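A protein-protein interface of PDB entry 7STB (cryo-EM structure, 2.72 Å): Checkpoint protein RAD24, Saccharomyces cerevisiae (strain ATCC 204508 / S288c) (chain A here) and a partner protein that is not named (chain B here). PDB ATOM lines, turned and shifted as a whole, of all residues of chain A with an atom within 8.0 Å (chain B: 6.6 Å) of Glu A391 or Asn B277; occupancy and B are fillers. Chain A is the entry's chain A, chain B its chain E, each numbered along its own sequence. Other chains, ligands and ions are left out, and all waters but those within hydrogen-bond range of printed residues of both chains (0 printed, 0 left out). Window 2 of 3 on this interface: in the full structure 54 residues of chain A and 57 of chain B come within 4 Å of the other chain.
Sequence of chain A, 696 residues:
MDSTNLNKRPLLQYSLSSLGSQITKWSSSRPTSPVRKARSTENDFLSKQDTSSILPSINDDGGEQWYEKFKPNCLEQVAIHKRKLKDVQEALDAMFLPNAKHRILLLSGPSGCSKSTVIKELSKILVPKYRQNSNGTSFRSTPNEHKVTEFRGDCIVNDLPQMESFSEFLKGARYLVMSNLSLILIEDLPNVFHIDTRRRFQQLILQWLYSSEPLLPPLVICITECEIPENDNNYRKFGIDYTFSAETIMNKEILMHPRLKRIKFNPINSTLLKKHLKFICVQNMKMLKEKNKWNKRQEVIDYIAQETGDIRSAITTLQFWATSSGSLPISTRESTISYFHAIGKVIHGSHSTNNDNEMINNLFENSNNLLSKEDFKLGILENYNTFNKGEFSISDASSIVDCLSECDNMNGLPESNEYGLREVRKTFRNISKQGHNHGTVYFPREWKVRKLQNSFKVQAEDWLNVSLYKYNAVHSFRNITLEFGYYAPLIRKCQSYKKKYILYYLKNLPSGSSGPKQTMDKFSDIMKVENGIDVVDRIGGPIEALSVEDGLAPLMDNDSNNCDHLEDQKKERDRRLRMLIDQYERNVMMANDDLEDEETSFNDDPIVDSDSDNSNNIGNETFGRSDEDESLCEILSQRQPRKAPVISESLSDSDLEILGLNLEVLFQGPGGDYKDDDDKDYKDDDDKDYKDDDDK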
ATOM      1  N   TYR A 384      10.964  -9.454  10.831  1.00  0.00           N
ATOM      2  CA  TYR A 384      10.878  -8.699  12.076  1.00  0.00           C
ATOM      3  C   TYR A 384      11.011  -7.197  11.857  1.00  0.00           C
ATOM      4  O   TYR A 384      10.666  -6.420  12.755  1.00  0.00           O
ATOM      5  CB  TYR A 384      11.952  -9.174  13.055  1.00  0.00           C
ATOM      6  CG  TYR A 384      13.294  -8.504  12.862  1.00  0.00           C
ATOM      7  CD1 TYR A 384      14.222  -9.014  11.968  1.00  0.00           C
ATOM      8  CD2 TYR A 384      13.632  -7.363  13.578  1.00  0.00           C
ATOM      9  CE1 TYR A 384      15.447  -8.407  11.786  1.00  0.00           C
ATOM     10  CE2 TYR A 384      14.853  -6.749  13.402  1.00  0.00           C
ATOM     11  CZ  TYR A 384      15.758  -7.275  12.506  1.00  0.00           C
ATOM     12  OH  TYR A 384      16.979  -6.668  12.329  1.00  0.00           O
ATOM     13  N   ASN A 385      11.500  -6.768  10.697  1.00  0.00           N
ATOM     14  CA  ASN A 385      11.751  -5.356  10.435  1.00  0.00           C
ATOM     15  C   ASN A 385      10.553  -4.636   9.829  1.00  0.00           C
ATOM     16  O   ASN A 385      10.652  -3.437   9.548  1.00  0.00           O
ATOM     17  CB  ASN A 385      12.954  -5.203   9.502  1.00  0.00           C
ATOM     18  CG  ASN A 385      12.753  -5.904   8.175  1.00  0.00           C
ATOM     19  OD1 ASN A 385      12.977  -7.109   8.056  1.00  0.00           O
ATOM     20  ND2 ASN A 385      12.326  -5.154   7.167  1.00  0.00           N
ATOM     21  N   THR A 386       9.435  -5.325   9.619  1.00  0.00           N
ATOM     22  CA  THR A 386       8.245  -4.713   9.041  1.00  0.00           C
ATOM     23  C   THR A 386       7.309  -4.134  10.093  1.00  0.00           C
ATOM     24  O   THR A 386       6.219  -3.672   9.741  1.00  0.00           O
ATOM     25  CB  THR A 386       7.478  -5.735   8.195  1.00  0.00           C
ATOM     26  OG1 THR A 386       7.003  -6.795   9.033  1.00  0.00           O
ATOM     27  CG2 THR A 386       8.371  -6.312   7.110  1.00  0.00           C
ATOM     28  N   PHE A 387       7.702  -4.150  11.368  1.00  0.00           N
ATOM     29  CA  PHE A 387       6.810  -3.701  12.431  1.00  0.00           C
ATOM     30  C   PHE A 387       6.319  -2.281  12.176  1.00  0.00           C
ATOM     31  O   PHE A 387       5.118  -2.048  11.999  1.00  0.00           O
ATOM     32  CB  PHE A 387       7.525  -3.792  13.781  1.00  0.00           C
ATOM     33  CG  PHE A 387       6.634  -3.512  14.957  1.00  0.00           C
ATOM     34  CD1 PHE A 387       5.419  -4.164  15.098  1.00  0.00           C
ATOM     35  CD2 PHE A 387       7.010  -2.594  15.923  1.00  0.00           C
ATOM     36  CE1 PHE A 387       4.599  -3.905  16.177  1.00  0.00           C
ATOM     37  CE2 PHE A 387       6.193  -2.332  17.006  1.00  0.00           C
ATOM     38  CZ  PHE A 387       4.986  -2.988  17.132  1.00  0.00           C
ATOM     39  N   ASN A 388       7.235  -1.317  12.152  1.00  0.00           N
ATOM     40  CA  ASN A 388       6.903   0.086  11.938  1.00  0.00           C
ATOM     41  C   ASN A 388       7.614   0.590  10.685  1.00  0.00           C
ATOM     42  O   ASN A 388       8.169   1.689  10.649  1.00  0.00           O
ATOM     43  CB  ASN A 388       7.257   0.908  13.180  1.00  0.00           C
ATOM     44  CG  ASN A 388       7.069   2.404  12.985  1.00  0.00           C
ATOM     45  OD1 ASN A 388       7.985   3.114  12.575  1.00  0.00           O
ATOM     46  ND2 ASN A 388       5.868   2.889  13.281  1.00  0.00           N
ATOM     47  N   LYS A 389       7.615  -0.232   9.635  1.00  0.00           N
ATOM     48  CA  LYS A 389       8.330   0.070   8.397  1.00  0.00           C
ATOM     49  C   LYS A 389       9.817   0.301   8.653  1.00  0.00           C
ATOM     50  O   LYS A 389      10.496   0.978   7.877  1.00  0.00           O
ATOM     51  CB  LYS A 389       7.715   1.275   7.678  1.00  0.00           C
ATOM     52  CG  LYS A 389       6.514   0.926   6.816  1.00  0.00           C
ATOM     53  CD  LYS A 389       6.141   2.067   5.887  1.00  0.00           C
ATOM     54  CE  LYS A 389       4.976   1.690   4.987  1.00  0.00           C
ATOM     55  NZ  LYS A 389       4.596   2.799   4.069  1.00  0.00           N
ATOM     56  N   GLY A 390      10.334  -0.262   9.744  1.00  0.00           N
ATOM     57  CA  GLY A 390      11.737  -0.165  10.074  1.00  0.00           C
ATOM     58  C   GLY A 390      12.110   0.989  10.979  1.00  0.00           C
ATOM     59  O   GLY A 390      13.223   0.992  11.521  1.00  0.00           O
ATOM     60  N   GLU A 391      11.223   1.967  11.169  1.00  0.00           N
ATOM     61  CA  GLU A 391      11.520   3.124  12.014  1.00  0.00           C
ATOM     62  C   GLU A 391      11.197   2.772  13.464  1.00  0.00           C
ATOM     63  O   GLU A 391      10.191   3.190  14.039  1.00  0.00           O
ATOM     64  CB  GLU A 391      10.751   4.350  11.541  1.00  0.00           C
ATOM     65  CG  GLU A 391      11.192   4.870  10.178  1.00  0.00           C
ATOM     66  CD  GLU A 391      10.560   4.120   9.023  1.00  0.00           C
ATOM     67  OE1 GLU A 391       9.722   3.228   9.273  1.00  0.00           O
ATOM     68  OE2 GLU A 391      10.900   4.424   7.861  1.00  0.00           O
ATOM     69  N   PHE A 392      12.085   1.980  14.060  1.00  0.00           N
ATOM     70  CA  PHE A 392      12.007   1.658  15.477  1.00  0.00           C
ATOM     71  C   PHE A 392      13.423   1.472  15.998  1.00  0.00           C
ATOM     72  O   PHE A 392      14.375   1.337  15.226  1.00  0.00           O
ATOM     73  CB  PHE A 392      11.145   0.414  15.738  1.00  0.00           C
ATOM     74  CG  PHE A 392      11.760  -0.873  15.261  1.00  0.00           C
ATOM     75  CD1 PHE A 392      12.611  -1.596  16.079  1.00  0.00           C
ATOM     76  CD2 PHE A 392      11.470  -1.367  14.001  1.00  0.00           C
ATOM     77  CE1 PHE A 392      13.172  -2.780  15.644  1.00  0.00           C
ATOM     78  CE2 PHE A 392      12.028  -2.552  13.561  1.00  0.00           C
ATOM     79  CZ  PHE A 392      12.880  -3.259  14.384  1.00  0.00           C
ATOM     80  N   SER A 393      13.552   1.473  17.324  1.00  0.00           N
ATOM     81  CA  SER A 393      14.868   1.474  17.950  1.00  0.00           C
ATOM     82  C   SER A 393      15.715   0.317  17.439  1.00  0.00           C
ATOM     83  O   SER A 393      15.268  -0.833  17.404  1.00  0.00           O
ATOM     84  CB  SER A 393      14.722   1.388  19.469  1.00  0.00           C
ATOM     85  OG  SER A 393      15.987   1.264  20.095  1.00  0.00           O
ATOM     86  N   ILE A 394      16.948   0.635  17.039  1.00  0.00           N
ATOM     87  CA  ILE A 394      17.865  -0.385  16.548  1.00  0.00           C
ATOM     88  C   ILE A 394      18.247  -1.368  17.647  1.00  0.00           C
ATOM     89  O   ILE A 394      18.639  -2.503  17.351  1.00  0.00           O
ATOM     90  CB  ILE A 394      19.114   0.283  15.940  1.00  0.00           C
ATOM     91  CG1 ILE A 394      19.986  -0.743  15.210  1.00  0.00           C
ATOM     92  CG2 ILE A 394      19.917   1.006  17.015  1.00  0.00           C
ATOM     93  CD1 ILE A 394      19.349  -1.323  13.968  1.00  0.00           C
ATOM     94  N   ASP A 396      16.252  -2.865  19.732  1.00  0.00           N
ATOM     95  CA  ASP A 396      15.317  -3.983  19.675  1.00  0.00           C
ATOM     96  C   ASP A 396      15.691  -4.953  18.562  1.00  0.00           C
ATOM     97  O   ASP A 396      15.657  -6.176  18.753  1.00  0.00           O
ATOM     98  CB  ASP A 396      13.893  -3.464  19.478  1.00  0.00           C
ATOM     99  CG  ASP A 396      13.552  -2.324  20.416  1.00  0.00           C
ATOM    100  OD1 ASP A 396      14.040  -2.331  21.566  1.00  0.00           O
ATOM    101  OD2 ASP A 396      12.798  -1.419  20.003  1.00  0.00           O
ATOM    102  N   ALA A 397      16.051  -4.427  17.390  1.00  0.00           N
ATOM    103  CA  ALA A 397      16.465  -5.289  16.289  1.00  0.00           C
ATOM    104  C   ALA A 397      17.716  -6.075  16.652  1.00  0.00           C
ATOM    105  O   ALA A 397      17.811  -7.276  16.372  1.00  0.00           O
ATOM    106  CB  ALA A 397      16.703  -4.454  15.032  1.00  0.00           C
ATOM    107  N   ILE A 431       7.444  -2.198  22.635  1.00  0.00           N
ATOM    108  CA  ILE A 431       7.405  -0.974  21.842  1.00  0.00           C
ATOM    109  C   ILE A 431       6.093  -0.825  21.077  1.00  0.00           C
ATOM    110  O   ILE A 431       5.999   0.019  20.180  1.00  0.00           O
ATOM    111  CB  ILE A 431       8.603  -0.906  20.881  1.00  0.00           C
ATOM    112  CG1 ILE A 431       8.577  -2.086  19.905  1.00  0.00           C
ATOM    113  CG2 ILE A 431       9.906  -0.892  21.664  1.00  0.00           C
ATOM    114  CD1 ILE A 431       9.659  -2.032  18.850  1.00  0.00           C
ATOM    115  N   LYS A 433       2.426   0.330  20.047  1.00  0.00           N
ATOM    116  CA  LYS A 433       1.630   1.532  20.246  1.00  0.00           C
ATOM    117  C   LYS A 433       0.523   1.564  19.203  1.00  0.00           C
ATOM    118  O   LYS A 433       0.582   0.871  18.185  1.00  0.00           O
ATOM    119  CB  LYS A 433       2.482   2.806  20.157  1.00  0.00           C
ATOM    120  CG  LYS A 433       3.583   2.899  21.202  1.00  0.00           C
ATOM    121  CD  LYS A 433       4.336   4.219  21.112  1.00  0.00           C
ATOM    122  CE  LYS A 433       5.176   4.304  19.846  1.00  0.00           C
ATOM    123  NZ  LYS A 433       5.973   5.562  19.790  1.00  0.00           N
ATOM    124  N   HIS A 436       0.823   2.765  14.582  1.00  0.00           N
ATOM    125  CA  HIS A 436       1.826   1.961  13.899  1.00  0.00           C
ATOM    126  C   HIS A 436       1.378   1.643  12.480  1.00  0.00           C
ATOM    127  O   HIS A 436       0.216   1.297  12.245  1.00  0.00           O
ATOM    128  CB  HIS A 436       2.095   0.660  14.663  1.00  0.00           C
ATOM    129  CG  HIS A 436       3.207   0.764  15.658  1.00  0.00           C
ATOM    130  ND1 HIS A 436       3.018   1.214  16.946  1.00  0.00           N
ATOM    131  CD2 HIS A 436       4.523   0.464  15.555  1.00  0.00           C
ATOM    132  CE1 HIS A 436       4.171   1.195  17.591  1.00  0.00           C
ATOM    133  NE2 HIS A 436       5.100   0.743  16.769  1.00  0.00           N
ATOM    134  N   ASN A 437       2.311   1.763  11.538  1.00  0.00           N
ATOM    135  CA  ASN A 437       2.102   1.382  10.147  1.00  0.00           C
ATOM    136  C   ASN A 437       3.134   0.330   9.777  1.00  0.00           C
ATOM    137  O   ASN A 437       4.333   0.526  10.003  1.00  0.00           O
ATOM    138  CB  ASN A 437       2.213   2.595   9.219  1.00  0.00           C
ATOM    139  CG  ASN A 437       1.652   2.325   7.838  1.00  0.00           C
ATOM    140  OD1 ASN A 437       1.154   1.235   7.559  1.00  0.00           O
ATOM    141  ND2 ASN A 437       1.732   3.321   6.962  1.00  0.00           N
ATOM    142  N   LYS B 269      29.062   1.830   4.342  1.00  0.00           N
ATOM    143  CA  LYS B 269      27.625   2.001   4.525  1.00  0.00           C
ATOM    144  C   LYS B 269      27.230   1.825   5.987  1.00  0.00           C
ATOM    145  O   LYS B 269      26.427   2.600   6.519  1.00  0.00           O
ATOM    146  CB  LYS B 269      26.870   1.008   3.643  1.00  0.00           C
ATOM    147  CG  LYS B 269      25.362   1.043   3.804  1.00  0.00           C
ATOM    148  CD  LYS B 269      24.687   0.122   2.802  1.00  0.00           C
ATOM    149  CE  LYS B 269      23.177   0.275   2.825  1.00  0.00           C
ATOM    150  NZ  LYS B 269      22.744   1.656   2.470  1.00  0.00           N
ATOM    151  N   SER B 275      21.127   2.402  11.242  1.00  0.00           N
ATOM    152  CA  SER B 275      19.674   2.349  11.320  1.00  0.00           C
ATOM    153  C   SER B 275      19.198   0.957  10.935  1.00  0.00           C
ATOM    154  O   SER B 275      19.934   0.165  10.344  1.00  0.00           O
ATOM    155  CB  SER B 275      19.021   3.397  10.410  1.00  0.00           C
ATOM    156  OG  SER B 275      19.035   2.977   9.057  1.00  0.00           O
ATOM    157  N   VAL B 276      17.943   0.665  11.286  1.00  0.00           N
ATOM    158  CA  VAL B 276      17.363  -0.631  10.946  1.00  0.00           C
ATOM    159  C   VAL B 276      17.337  -0.820   9.436  1.00  0.00           C
ATOM    160  O   VAL B 276      17.731  -1.873   8.920  1.00  0.00           O
ATOM    161  CB  VAL B 276      15.955  -0.764  11.557  1.00  0.00           C
ATOM    162  CG1 VAL B 276      15.218  -1.950  10.950  1.00  0.00           C
ATOM    163  CG2 VAL B 276      16.042  -0.904  13.067  1.00  0.00           C
ATOM    164  N   ASN B 277      16.882   0.199   8.701  1.00  0.00           N
ATOM    165  CA  ASN B 277      16.836   0.096   7.247  1.00  0.00           C
ATOM    166  C   ASN B 277      18.225  -0.154   6.672  1.00  0.00           C
ATOM    167  O   ASN B 277      18.373  -0.862   5.669  1.00  0.00           O
ATOM    168  CB  ASN B 277      16.227   1.365   6.653  1.00  0.00           C
ATOM    169  CG  ASN B 277      14.724   1.437   6.846  1.00  0.00           C
ATOM    170  OD1 ASN B 277      14.015   0.447   6.664  1.00  0.00           O
ATOM    171  ND2 ASN B 277      14.232   2.612   7.222  1.00  0.00           N
ATOM    172  N   SER B 278      19.256   0.419   7.295  1.00  0.00           N
ATOM    173  CA  SER B 278      20.620   0.137   6.865  1.00  0.00           C
ATOM    174  C   SER B 278      20.951  -1.339   7.043  1.00  0.00           C
ATOM    175  O   SER B 278      21.589  -1.951   6.179  1.00  0.00           O
ATOM    176  CB  SER B 278      21.604   1.009   7.645  1.00  0.00           C
ATOM    177  OG  SER B 278      22.910   0.909   7.108  1.00  0.00           O
ATOM    178  N   LEU B 279      20.523  -1.930   8.162  1.00  0.00           N
ATOM    179  CA  LEU B 279      20.722  -3.360   8.367  1.00  0.00           C
ATOM    180  C   LEU B 279      20.000  -4.169   7.296  1.00  0.00           C
ATOM    181  O   LEU B 279      20.547  -5.142   6.761  1.00  0.00           O
ATOM    182  CB  LEU B 279      20.229  -3.757   9.759  1.00  0.00           C
ATOM    183  CG  LEU B 279      20.421  -5.216  10.174  1.00  0.00           C
ATOM    184  CD1 LEU B 279      21.897  -5.575  10.225  1.00  0.00           C
ATOM    185  CD2 LEU B 279      19.759  -5.471  11.516  1.00  0.00           C
ATOM    186  N   ILE B 280      18.769  -3.775   6.969  1.00  0.00           N
ATOM    187  CA  ILE B 280      18.010  -4.499   5.956  1.00  0.00           C
ATOM    188  C   ILE B 280      18.729  -4.432   4.616  1.00  0.00           C
ATOM    189  O   ILE B 280      18.824  -5.431   3.893  1.00  0.00           O
ATOM    190  CB  ILE B 280      16.580  -3.937   5.853  1.00  0.00           C
ATOM    191  CG1 ILE B 280      15.907  -3.859   7.230  1.00  0.00           C
ATOM    192  CG2 ILE B 280      15.747  -4.791   4.909  1.00  0.00           C
ATOM    193  CD1 ILE B 280      15.944  -5.130   8.054  1.00  0.00           C
ATOM    194  N   GLU B 281      19.243  -3.253   4.263  1.00  0.00           N
ATOM    195  CA  GLU B 281      19.968  -3.106   3.004  1.00  0.00           C
ATOM    196  C   GLU B 281      21.241  -3.943   2.996  1.00  0.00           C
ATOM    197  O   GLU B 281      21.557  -4.590   1.991  1.00  0.00           O
ATOM    198  CB  GLU B 281      20.289  -1.632   2.760  1.00  0.00           C
ATOM    199  CG  GLU B 281      19.072  -0.798   2.390  1.00  0.00           C
ATOM    200  CD  GLU B 281      19.274   0.686   2.637  1.00  0.00           C
ATOM    201  OE1 GLU B 281      20.389   1.081   3.035  1.00  0.00           O
ATOM    202  OE2 GLU B 281      18.312   1.457   2.434  1.00  0.00           O
ATOM    203  N   CYS B 282      21.984  -3.944   4.105  1.00  0.00           N
ATOM    204  CA  CYS B 282      23.192  -4.759   4.191  1.00  0.00           C
ATOM    205  C   CYS B 282      22.885  -6.249   4.120  1.00  0.00           C
ATOM    206  O   CYS B 282      23.754  -7.036   3.718  1.00  0.00           O
ATOM    207  CB  CYS B 282      23.942  -4.446   5.487  1.00  0.00           C
ATOM    208  SG  CYS B 282      24.694  -2.802   5.539  1.00  0.00           S
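The backbone carbonyl oxygen (O) of Glu A391 sits close to the side-chain amide oxygen (OD1) of Asn A388 (2.6 Å).
The backbone carbonyl oxygen (O) of Asn A385 lies within hydrogen-bond range of the backbone NH (N) of Gly A390 (3.2 Å).
OG of Ser B275 sits at hydrogen-bond distance from N of Ser B278 (3.1 Å).
The backbone NH of Lys A389 is in hydrogen-bond range of the backbone carbonyl oxygen of Asn A437.
Among the printed residues, pairs that only touch across the chains: Tyr A384 with Leu B279 (3.1 Å), Gly A390 with Val B276 (3.2 Å), Asn A385 with Ile B280 (3.3 Å), Ile A394 with Val B276 (3.5 Å), Phe A392 with Val B276 (3.5 Å), Lys A389 with Asn B277 (3.8 Å), Ile A394 with Ser B275 (3.8 Å) and Glu A391 with Asn B277 (3.8 Å).
Thr A386 touches none of the printed residues of chain B.
Printed residues of chain B within 4 Å of Gly A390: Val B276 (3.2 Å).
Glu A391 touches one residue of chain B.
Of the printed residues of chain B, Phe A392 touches Val B276.
Asp A396 touches none of the printed residues of chain B.
Of chain A, only Lys A389 (3.8 Å) and Glu A391 (3.8 Å) come within 4 Å of Asn B277.
Of the 17 printed residues of chain A, 7 touch a printed residue of chain B.
Hydrophobic or aromatic side chains of chain A that line the printed part of chain B: Tyr A384 and Ile A394.
Along chain A the printed residues that touch a printed residue of chain B span positions 384 to 394.
Hydrophobic or aromatic side chains of chain B within 4 Å of the printed part of chain A: Val B276, Leu B279 and Ile B280.
Along chain B the printed residues that touch a printed residue of chain A span positions 275 to 280.
Among the printed residues, 8 pairs touch across the chains.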
